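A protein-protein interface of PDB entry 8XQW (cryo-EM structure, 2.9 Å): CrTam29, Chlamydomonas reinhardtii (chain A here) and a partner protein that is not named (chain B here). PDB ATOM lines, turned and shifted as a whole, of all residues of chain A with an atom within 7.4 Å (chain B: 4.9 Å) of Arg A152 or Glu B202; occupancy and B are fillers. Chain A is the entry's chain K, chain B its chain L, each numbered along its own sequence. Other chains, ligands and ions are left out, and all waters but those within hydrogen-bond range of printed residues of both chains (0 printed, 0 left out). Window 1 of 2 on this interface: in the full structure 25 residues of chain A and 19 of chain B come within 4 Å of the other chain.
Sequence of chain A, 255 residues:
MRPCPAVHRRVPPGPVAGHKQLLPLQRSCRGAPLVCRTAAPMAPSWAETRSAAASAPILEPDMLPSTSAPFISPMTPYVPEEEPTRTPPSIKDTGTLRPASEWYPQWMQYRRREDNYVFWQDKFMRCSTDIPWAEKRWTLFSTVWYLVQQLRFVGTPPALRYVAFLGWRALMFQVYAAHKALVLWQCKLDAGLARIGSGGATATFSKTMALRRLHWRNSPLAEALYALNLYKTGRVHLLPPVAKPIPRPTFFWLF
NH1 of Arg A161 sits close to OE1 of Glu B202, 2.2 Å away. NH2 of Arg A152 lies within salt-bridge range of OE2 of Glu B202 (3.8 Å).
The backbone carbonyl oxygen (O) of Thr A156 lies within hydrogen-bond range of the guanidinium group (NE) of Arg A161. The backbone carbonyl oxygen of Phe A153 sits at hydrogen-bond distance from the guanidinium group of Arg A161. NE of Arg A161 sits at hydrogen-bond distance from O of Arg A152 (3.1 Å). The side-chain carboxylate (OE2) of Glu B202 is in salt-bridge range of the guanidinium group (NE) of Arg B205 (3.1 Å).
Among the printed residues, pairs that only touch across the chains: Trp A103 with Met B200, Trp A103 with Glu B204, Phe A153 with Glu B202, Phe A153 with Ile B206, Pro A158 with Phe B198, Arg A161 with Phe B198, Tyr A162 with Phe B198 and Phe A165 with Phe B198.
Of the printed residues of chain B, Trp A103 touches Met B200 and Glu B204. Tyr A146 touches none of the printed residues of chain B. Of chain B, only Glu B202 comes within 4 Å of Arg A152. Of the printed residues of chain B, Phe A165 touches Phe B198 (3.8 Å). Of the printed residues of chain A, Met B200 touches Trp A103. The nearest residue of chain A that does not touch Glu B202 is Phe A165 (6.4 Å). The nearest printed residue of chain A that does not touch Met B200 is Arg A161 (9.2 Å).
Printed residues of chain A that touch a printed residue of chain B: Trp A103, Arg A152, Phe A153, Pro A158, Arg A161, Tyr A162 and Phe A165. Hydrophobic or aromatic side chains of chain A that line the printed part of chain B: Trp A103, Phe A153, Tyr A162 and Phe A165. Along chain A the printed residues that touch a printed residue of chain B span positions 103 to 165. Of the 9 printed residues of chain B, 5 touch a printed residue of chain A. Along chain B the printed residues that touch a printed residue of chain A span positions 198 to 206. Among the printed residues, 10 pairs touch across the chains.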
ATOM      1  N   TRP A 103     -20.192 -29.012 -20.804  1.00  0.00           N
ATOM      2  CA  TRP A 103     -20.379 -28.057 -19.689  1.00  0.00           C
ATOM      3  C   TRP A 103     -20.716 -28.764 -18.389  1.00  0.00           C
ATOM      4  O   TRP A 103     -19.844 -28.805 -17.529  1.00  0.00           O
ATOM      5  CB  TRP A 103     -21.457 -27.042 -20.042  1.00  0.00           C
ATOM      6  CG  TRP A 103     -21.506 -25.856 -19.126  1.00  0.00           C
ATOM      7  CD1 TRP A 103     -22.618 -25.291 -18.586  1.00  0.00           C
ATOM      8  CD2 TRP A 103     -20.387 -25.080 -18.663  1.00  0.00           C
ATOM      9  NE1 TRP A 103     -22.272 -24.225 -17.806  1.00  0.00           N
ATOM     10  CE2 TRP A 103     -20.915 -24.071 -17.836  1.00  0.00           C
ATOM     11  CE3 TRP A 103     -19.007 -25.140 -18.864  1.00  0.00           C
ATOM     12  CZ2 TRP A 103     -20.110 -23.128 -17.212  1.00  0.00           C
ATOM     13  CZ3 TRP A 103     -18.211 -24.208 -18.247  1.00  0.00           C
ATOM     14  CH2 TRP A 103     -18.761 -23.218 -17.439  1.00  0.00           C
ATOM     15  N   TRP A 145       7.216 -22.829 -24.246  1.00  0.00           N
ATOM     16  CA  TRP A 145       5.842 -23.276 -24.180  1.00  0.00           C
ATOM     17  C   TRP A 145       4.891 -22.101 -24.055  1.00  0.00           C
ATOM     18  O   TRP A 145       3.746 -22.183 -24.510  1.00  0.00           O
ATOM     19  CB  TRP A 145       5.660 -24.244 -23.027  1.00  0.00           C
ATOM     20  CG  TRP A 145       4.403 -24.943 -23.144  1.00  0.00           C
ATOM     21  CD1 TRP A 145       3.283 -24.725 -22.430  1.00  0.00           C
ATOM     22  CD2 TRP A 145       4.093 -25.959 -24.081  1.00  0.00           C
ATOM     23  NE1 TRP A 145       2.286 -25.550 -22.851  1.00  0.00           N
ATOM     24  CE2 TRP A 145       2.764 -26.322 -23.871  1.00  0.00           C
ATOM     25  CE3 TRP A 145       4.815 -26.601 -25.081  1.00  0.00           C
ATOM     26  CZ2 TRP A 145       2.142 -27.299 -24.611  1.00  0.00           C
ATOM     27  CZ3 TRP A 145       4.198 -27.564 -25.814  1.00  0.00           C
ATOM     28  CH2 TRP A 145       2.875 -27.906 -25.579  1.00  0.00           C
ATOM     29  N   TYR A 146       5.334 -20.998 -23.456  1.00  0.00           N
ATOM     30  CA  TYR A 146       4.480 -19.822 -23.427  1.00  0.00           C
ATOM     31  C   TYR A 146       4.115 -19.377 -24.827  1.00  0.00           C
ATOM     32  O   TYR A 146       2.974 -19.000 -25.078  1.00  0.00           O
ATOM     33  CB  TYR A 146       5.147 -18.675 -22.681  1.00  0.00           C
ATOM     34  CG  TYR A 146       4.306 -17.433 -22.693  1.00  0.00           C
ATOM     35  CD1 TYR A 146       3.281 -17.267 -21.802  1.00  0.00           C
ATOM     36  CD2 TYR A 146       4.524 -16.438 -23.611  1.00  0.00           C
ATOM     37  CE1 TYR A 146       2.515 -16.155 -21.822  1.00  0.00           C
ATOM     38  CE2 TYR A 146       3.760 -15.320 -23.632  1.00  0.00           C
ATOM     39  CZ  TYR A 146       2.755 -15.189 -22.741  1.00  0.00           C
ATOM     40  OH  TYR A 146       1.992 -14.063 -22.770  1.00  0.00           O
ATOM     41  N   LEU A 147       5.064 -19.408 -25.754  1.00  0.00           N
ATOM     42  CA  LEU A 147       4.776 -18.959 -27.110  1.00  0.00           C
ATOM     43  C   LEU A 147       3.847 -19.918 -27.820  1.00  0.00           C
ATOM     44  O   LEU A 147       2.945 -19.491 -28.547  1.00  0.00           O
ATOM     45  CB  LEU A 147       6.062 -18.809 -27.894  1.00  0.00           C
ATOM     46  CG  LEU A 147       6.980 -17.710 -27.422  1.00  0.00           C
ATOM     47  CD1 LEU A 147       8.244 -17.848 -28.169  1.00  0.00           C
ATOM     48  CD2 LEU A 147       6.344 -16.398 -27.695  1.00  0.00           C
ATOM     49  N   VAL A 148       4.046 -21.218 -27.626  1.00  0.00           N
ATOM     50  CA  VAL A 148       3.103 -22.175 -28.214  1.00  0.00           C
ATOM     51  C   VAL A 148       1.684 -21.884 -27.742  1.00  0.00           C
ATOM     52  O   VAL A 148       0.742 -21.756 -28.540  1.00  0.00           O
ATOM     53  CB  VAL A 148       3.505 -23.615 -27.871  1.00  0.00           C
ATOM     54  CG1 VAL A 148       2.459 -24.549 -28.360  1.00  0.00           C
ATOM     55  CG2 VAL A 148       4.813 -23.957 -28.496  1.00  0.00           C
ATOM     56  N   GLN A 149       1.512 -21.763 -26.431  1.00  0.00           N
ATOM     57  CA  GLN A 149       0.183 -21.563 -25.876  1.00  0.00           C
ATOM     58  C   GLN A 149      -0.403 -20.216 -26.248  1.00  0.00           C
ATOM     59  O   GLN A 149      -1.610 -20.112 -26.469  1.00  0.00           O
ATOM     60  CB  GLN A 149       0.238 -21.708 -24.371  1.00  0.00           C
ATOM     61  CG  GLN A 149      -0.914 -22.451 -23.814  1.00  0.00           C
ATOM     62  CD  GLN A 149      -0.748 -23.918 -23.959  1.00  0.00           C
ATOM     63  OE1 GLN A 149       0.282 -24.386 -24.407  1.00  0.00           O
ATOM     64  NE2 GLN A 149      -1.766 -24.664 -23.592  1.00  0.00           N
ATOM     65  N   GLN A 150       0.412 -19.172 -26.304  1.00  0.00           N
ATOM     66  CA  GLN A 150      -0.114 -17.869 -26.668  1.00  0.00           C
ATOM     67  C   GLN A 150      -0.547 -17.839 -28.119  1.00  0.00           C
ATOM     68  O   GLN A 150      -1.527 -17.174 -28.448  1.00  0.00           O
ATOM     69  CB  GLN A 150       0.917 -16.786 -26.396  1.00  0.00           C
ATOM     70  CG  GLN A 150       1.215 -15.918 -27.576  1.00  0.00           C
ATOM     71  CD  GLN A 150       0.639 -14.545 -27.432  1.00  0.00           C
ATOM     72  OE1 GLN A 150       0.243 -13.922 -28.407  1.00  0.00           O
ATOM     73  NE2 GLN A 150       0.595 -14.053 -26.212  1.00  0.00           N
ATOM     74  N   LEU A 151       0.145 -18.562 -28.994  1.00  0.00           N
ATOM     75  CA  LEU A 151      -0.373 -18.735 -30.342  1.00  0.00           C
ATOM     76  C   LEU A 151      -1.751 -19.367 -30.300  1.00  0.00           C
ATOM     77  O   LEU A 151      -2.702 -18.824 -30.859  1.00  0.00           O
ATOM     78  CB  LEU A 151       0.577 -19.581 -31.174  1.00  0.00           C
ATOM     79  CG  LEU A 151       0.269 -19.616 -32.662  1.00  0.00           C
ATOM     80  CD1 LEU A 151       0.417 -18.244 -33.240  1.00  0.00           C
ATOM     81  CD2 LEU A 151       1.198 -20.563 -33.353  1.00  0.00           C
ATOM     82  N   ARG A 152      -1.888 -20.490 -29.595  1.00  0.00           N
ATOM     83  CA  ARG A 152      -3.172 -21.192 -29.593  1.00  0.00           C
ATOM     84  C   ARG A 152      -4.299 -20.339 -29.019  1.00  0.00           C
ATOM     85  O   ARG A 152      -5.454 -20.478 -29.424  1.00  0.00           O
ATOM     86  CB  ARG A 152      -3.059 -22.508 -28.829  1.00  0.00           C
ATOM     87  CG  ARG A 152      -4.021 -22.636 -27.692  1.00  0.00           C
ATOM     88  CD  ARG A 152      -4.721 -23.951 -27.682  1.00  0.00           C
ATOM     89  NE  ARG A 152      -4.435 -24.720 -26.478  1.00  0.00           N
ATOM     90  CZ  ARG A 152      -5.358 -25.362 -25.774  1.00  0.00           C
ATOM     91  NH1 ARG A 152      -5.024 -26.047 -24.698  1.00  0.00           N
ATOM     92  NH2 ARG A 152      -6.620 -25.309 -26.146  1.00  0.00           N
ATOM     93  N   PHE A 153      -3.999 -19.458 -28.070  1.00  0.00           N
ATOM     94  CA  PHE A 153      -5.069 -18.746 -27.377  1.00  0.00           C
ATOM     95  C   PHE A 153      -5.350 -17.356 -27.916  1.00  0.00           C
ATOM     96  O   PHE A 153      -6.466 -16.868 -27.740  1.00  0.00           O
ATOM     97  CB  PHE A 153      -4.765 -18.606 -25.885  1.00  0.00           C
ATOM     98  CG  PHE A 153      -5.081 -19.822 -25.093  1.00  0.00           C
ATOM     99  CD1 PHE A 153      -6.288 -20.446 -25.223  1.00  0.00           C
ATOM    100  CD2 PHE A 153      -4.169 -20.348 -24.223  1.00  0.00           C
ATOM    101  CE1 PHE A 153      -6.566 -21.560 -24.510  1.00  0.00           C
ATOM    102  CE2 PHE A 153      -4.448 -21.461 -23.518  1.00  0.00           C
ATOM    103  CZ  PHE A 153      -5.641 -22.064 -23.662  1.00  0.00           C
ATOM    104  N   VAL A 154      -4.386 -16.685 -28.541  1.00  0.00           N
ATOM    105  CA  VAL A 154      -4.599 -15.301 -28.950  1.00  0.00           C
ATOM    106  C   VAL A 154      -4.365 -15.139 -30.444  1.00  0.00           C
ATOM    107  O   VAL A 154      -4.864 -14.196 -31.061  1.00  0.00           O
ATOM    108  CB  VAL A 154      -3.693 -14.350 -28.155  1.00  0.00           C
ATOM    109  CG1 VAL A 154      -4.094 -12.930 -28.385  1.00  0.00           C
ATOM    110  CG2 VAL A 154      -3.766 -14.661 -26.691  1.00  0.00           C
ATOM    111  N   GLY A 155      -3.601 -16.044 -31.041  1.00  0.00           N
ATOM    112  CA  GLY A 155      -3.304 -15.903 -32.445  1.00  0.00           C
ATOM    113  C   GLY A 155      -4.099 -16.782 -33.360  1.00  0.00           C
ATOM    114  O   GLY A 155      -3.864 -16.769 -34.567  1.00  0.00           O
ATOM    115  N   THR A 156      -5.013 -17.539 -32.839  1.00  0.00           N
ATOM    116  CA  THR A 156      -5.864 -18.367 -33.656  1.00  0.00           C
ATOM    117  C   THR A 156      -7.321 -18.015 -33.408  1.00  0.00           C
ATOM    118  O   THR A 156      -7.723 -17.854 -32.255  1.00  0.00           O
ATOM    119  CB  THR A 156      -5.628 -19.840 -33.343  1.00  0.00           C
ATOM    120  OG1 THR A 156      -4.231 -20.113 -33.425  1.00  0.00           O
ATOM    121  CG2 THR A 156      -6.339 -20.718 -34.320  1.00  0.00           C
ATOM    122  N   PRO A 157      -8.128 -17.864 -34.461  1.00  0.00           N
ATOM    123  CA  PRO A 157      -9.506 -17.434 -34.265  1.00  0.00           C
ATOM    124  C   PRO A 157     -10.334 -18.530 -33.624  1.00  0.00           C
ATOM    125  O   PRO A 157     -10.185 -19.713 -33.962  1.00  0.00           O
ATOM    126  CB  PRO A 157      -9.987 -17.140 -35.695  1.00  0.00           C
ATOM    127  CG  PRO A 157      -9.097 -17.905 -36.543  1.00  0.00           C
ATOM    128  CD  PRO A 157      -7.776 -17.904 -35.885  1.00  0.00           C
ATOM    129  N   PRO A 158     -11.250 -18.179 -32.724  1.00  0.00           N
ATOM    130  CA  PRO A 158     -12.027 -19.206 -32.015  1.00  0.00           C
ATOM    131  C   PRO A 158     -12.837 -20.127 -32.908  1.00  0.00           C
ATOM    132  O   PRO A 158     -13.201 -21.217 -32.465  1.00  0.00           O
ATOM    133  CB  PRO A 158     -12.941 -18.380 -31.110  1.00  0.00           C
ATOM    134  CG  PRO A 158     -12.257 -17.100 -30.948  1.00  0.00           C
ATOM    135  CD  PRO A 158     -11.512 -16.834 -32.202  1.00  0.00           C
ATOM    136  N   ARG A 161     -10.602 -23.057 -33.915  1.00  0.00           N
ATOM    137  CA  ARG A 161     -10.429 -23.827 -32.697  1.00  0.00           C
ATOM    138  C   ARG A 161     -11.665 -24.654 -32.399  1.00  0.00           C
ATOM    139  O   ARG A 161     -11.559 -25.793 -31.939  1.00  0.00           O
ATOM    140  CB  ARG A 161     -10.117 -22.890 -31.546  1.00  0.00           C
ATOM    141  CG  ARG A 161      -8.739 -22.316 -31.601  1.00  0.00           C
ATOM    142  CD  ARG A 161      -8.349 -21.798 -30.257  1.00  0.00           C
ATOM    143  NE  ARG A 161      -8.506 -20.359 -30.158  1.00  0.00           N
ATOM    144  CZ  ARG A 161      -8.996 -19.744 -29.096  1.00  0.00           C
ATOM    145  NH1 ARG A 161      -9.375 -20.451 -28.054  1.00  0.00           N
ATOM    146  NH2 ARG A 161      -9.103 -18.430 -29.069  1.00  0.00           N
ATOM    147  N   TYR A 162     -12.847 -24.112 -32.677  1.00  0.00           N
ATOM    148  CA  TYR A 162     -14.072 -24.861 -32.435  1.00  0.00           C
ATOM    149  C   TYR A 162     -14.181 -26.061 -33.356  1.00  0.00           C
ATOM    150  O   TYR A 162     -14.566 -27.155 -32.924  1.00  0.00           O
ATOM    151  CB  TYR A 162     -15.272 -23.951 -32.609  1.00  0.00           C
ATOM    152  CG  TYR A 162     -16.588 -24.631 -32.413  1.00  0.00           C
ATOM    153  CD1 TYR A 162     -16.812 -25.451 -31.335  1.00  0.00           C
ATOM    154  CD2 TYR A 162     -17.615 -24.431 -33.298  1.00  0.00           C
ATOM    155  CE1 TYR A 162     -18.013 -26.061 -31.163  1.00  0.00           C
ATOM    156  CE2 TYR A 162     -18.809 -25.034 -33.128  1.00  0.00           C
ATOM    157  CZ  TYR A 162     -19.004 -25.845 -32.063  1.00  0.00           C
ATOM    158  OH  TYR A 162     -20.215 -26.450 -31.906  1.00  0.00           O
ATOM    159  N   PHE A 165     -11.895 -28.667 -32.149  1.00  0.00           N
ATOM    160  CA  PHE A 165     -12.457 -29.264 -30.946  1.00  0.00           C
ATOM    161  C   PHE A 165     -13.454 -30.361 -31.288  1.00  0.00           C
ATOM    162  O   PHE A 165     -13.395 -31.460 -30.726  1.00  0.00           O
ATOM    163  CB  PHE A 165     -13.105 -28.164 -30.118  1.00  0.00           C
ATOM    164  CG  PHE A 165     -13.897 -28.650 -28.958  1.00  0.00           C
ATOM    165  CD1 PHE A 165     -13.269 -29.063 -27.806  1.00  0.00           C
ATOM    166  CD2 PHE A 165     -15.271 -28.650 -28.999  1.00  0.00           C
ATOM    167  CE1 PHE A 165     -13.998 -29.494 -26.738  1.00  0.00           C
ATOM    168  CE2 PHE A 165     -15.997 -29.084 -27.928  1.00  0.00           C
ATOM    169  CZ  PHE A 165     -15.360 -29.503 -26.800  1.00  0.00           C
ATOM    170  N   PHE B 198     -18.633 -24.142 -25.684  1.00  0.00           N
ATOM    171  CA  PHE B 198     -17.228 -24.137 -26.064  1.00  0.00           C
ATOM    172  C   PHE B 198     -16.558 -22.838 -25.656  1.00  0.00           C
ATOM    173  O   PHE B 198     -15.451 -22.844 -25.114  1.00  0.00           O
ATOM    174  CB  PHE B 198     -17.058 -24.358 -27.558  1.00  0.00           C
ATOM    175  CG  PHE B 198     -15.657 -24.164 -28.018  1.00  0.00           C
ATOM    176  CD1 PHE B 198     -14.702 -25.113 -27.756  1.00  0.00           C
ATOM    177  CD2 PHE B 198     -15.281 -23.020 -28.677  1.00  0.00           C
ATOM    178  CE1 PHE B 198     -13.419 -24.929 -28.153  1.00  0.00           C
ATOM    179  CE2 PHE B 198     -13.996 -22.836 -29.068  1.00  0.00           C
ATOM    180  CZ  PHE B 198     -13.068 -23.794 -28.812  1.00  0.00           C
ATOM    181  N   LEU B 199     -17.203 -21.709 -25.922  1.00  0.00           N
ATOM    182  CA  LEU B 199     -16.596 -20.433 -25.572  1.00  0.00           C
ATOM    183  C   LEU B 199     -16.355 -20.313 -24.077  1.00  0.00           C
ATOM    184  O   LEU B 199     -15.328 -19.778 -23.655  1.00  0.00           O
ATOM    185  CB  LEU B 199     -17.472 -19.292 -26.052  1.00  0.00           C
ATOM    186  CG  LEU B 199     -17.216 -18.772 -27.452  1.00  0.00           C
ATOM    187  CD1 LEU B 199     -17.958 -17.494 -27.602  1.00  0.00           C
ATOM    188  CD2 LEU B 199     -15.757 -18.539 -27.659  1.00  0.00           C
ATOM    189  N   MET B 200     -17.270 -20.820 -23.258  1.00  0.00           N
ATOM    190  CA  MET B 200     -17.082 -20.711 -21.817  1.00  0.00           C
ATOM    191  C   MET B 200     -15.988 -21.643 -21.312  1.00  0.00           C
ATOM    192  O   MET B 200     -15.197 -21.264 -20.440  1.00  0.00           O
ATOM    193  CB  MET B 200     -18.395 -20.988 -21.104  1.00  0.00           C
ATOM    194  CG  MET B 200     -19.309 -19.793 -21.071  1.00  0.00           C
ATOM    195  SD  MET B 200     -20.643 -19.975 -19.892  1.00  0.00           S
ATOM    196  CE  MET B 200     -21.426 -21.456 -20.508  1.00  0.00           C
ATOM    197  N   SER B 201     -15.908 -22.857 -21.854  1.00  0.00           N
ATOM    198  CA  SER B 201     -14.798 -23.729 -21.496  1.00  0.00           C
ATOM    199  C   SER B 201     -13.459 -23.131 -21.892  1.00  0.00           C
ATOM    200  O   SER B 201     -12.486 -23.237 -21.137  1.00  0.00           O
ATOM    201  CB  SER B 201     -14.974 -25.087 -22.141  1.00  0.00           C
ATOM    202  OG  SER B 201     -16.217 -25.638 -21.776  1.00  0.00           O
ATOM    203  N   GLU B 202     -13.386 -22.486 -23.053  1.00  0.00           N
ATOM    204  CA  GLU B 202     -12.148 -21.819 -23.433  1.00  0.00           C
ATOM    205  C   GLU B 202     -11.832 -20.670 -22.497  1.00  0.00           C
ATOM    206  O   GLU B 202     -10.664 -20.405 -22.208  1.00  0.00           O
ATOM    207  CB  GLU B 202     -12.226 -21.316 -24.864  1.00  0.00           C
ATOM    208  CG  GLU B 202     -11.973 -22.377 -25.876  1.00  0.00           C
ATOM    209  CD  GLU B 202     -10.513 -22.735 -26.009  1.00  0.00           C
ATOM    210  OE1 GLU B 202      -9.717 -21.862 -26.393  1.00  0.00           O
ATOM    211  OE2 GLU B 202     -10.163 -23.900 -25.741  1.00  0.00           O
ATOM    212  N   GLY B 203     -12.851 -19.961 -22.024  1.00  0.00           N
ATOM    213  CA  GLY B 203     -12.607 -18.923 -21.041  1.00  0.00           C
ATOM    214  C   GLY B 203     -11.963 -19.456 -19.779  1.00  0.00           C
ATOM    215  O   GLY B 203     -11.005 -18.879 -19.264  1.00  0.00           O
ATOM    216  N   GLU B 204     -12.476 -20.568 -19.267  1.00  0.00           N
ATOM    217  CA  GLU B 204     -11.866 -21.172 -18.086  1.00  0.00           C
ATOM    218  C   GLU B 204     -10.437 -21.609 -18.352  1.00  0.00           C
ATOM    219  O   GLU B 204      -9.563 -21.457 -17.495  1.00  0.00           O
ATOM    220  CB  GLU B 204     -12.679 -22.365 -17.625  1.00  0.00           C
ATOM    221  CG  GLU B 204     -13.825 -22.000 -16.752  1.00  0.00           C
ATOM    222  CD  GLU B 204     -15.053 -22.805 -17.076  1.00  0.00           C
ATOM    223  OE1 GLU B 204     -16.147 -22.214 -17.133  1.00  0.00           O
ATOM    224  OE2 GLU B 204     -14.924 -24.030 -17.274  1.00  0.00           O
ATOM    225  N   ARG B 205     -10.184 -22.185 -19.525  1.00  0.00           N
ATOM    226  CA  ARG B 205      -8.827 -22.609 -19.844  1.00  0.00           C
ATOM    227  C   ARG B 205      -7.872 -21.428 -19.907  1.00  0.00           C
ATOM    228  O   ARG B 205      -6.729 -21.518 -19.450  1.00  0.00           O
ATOM    229  CB  ARG B 205      -8.822 -23.377 -21.154  1.00  0.00           C
ATOM    230  CG  ARG B 205      -8.892 -24.851 -20.941  1.00  0.00           C
ATOM    231  CD  ARG B 205      -8.606 -25.591 -22.196  1.00  0.00           C
ATOM    232  NE  ARG B 205      -9.707 -25.499 -23.139  1.00  0.00           N
ATOM    233  CZ  ARG B 205     -10.757 -26.304 -23.131  1.00  0.00           C
ATOM    234  NH1 ARG B 205     -10.850 -27.259 -22.224  1.00  0.00           N
ATOM    235  NH2 ARG B 205     -11.714 -26.151 -24.028  1.00  0.00           N
ATOM    236  N   ILE B 206      -8.322 -20.307 -20.460  1.00  0.00           N
ATOM    237  CA  ILE B 206      -7.477 -19.124 -20.520  1.00  0.00           C
ATOM    238  C   ILE B 206      -7.193 -18.600 -19.126  1.00  0.00           C
ATOM    239  O   ILE B 206      -6.080 -18.159 -18.835  1.00  0.00           O
ATOM    240  CB  ILE B 206      -8.133 -18.046 -21.388  1.00  0.00           C
ATOM    241  CG1 ILE B 206      -8.168 -18.481 -22.835  1.00  0.00           C
ATOM    242  CG2 ILE B 206      -7.373 -16.777 -21.296  1.00  0.00           C
ATOM    243  CD1 ILE B 206      -8.760 -17.467 -23.725  1.00  0.00           C
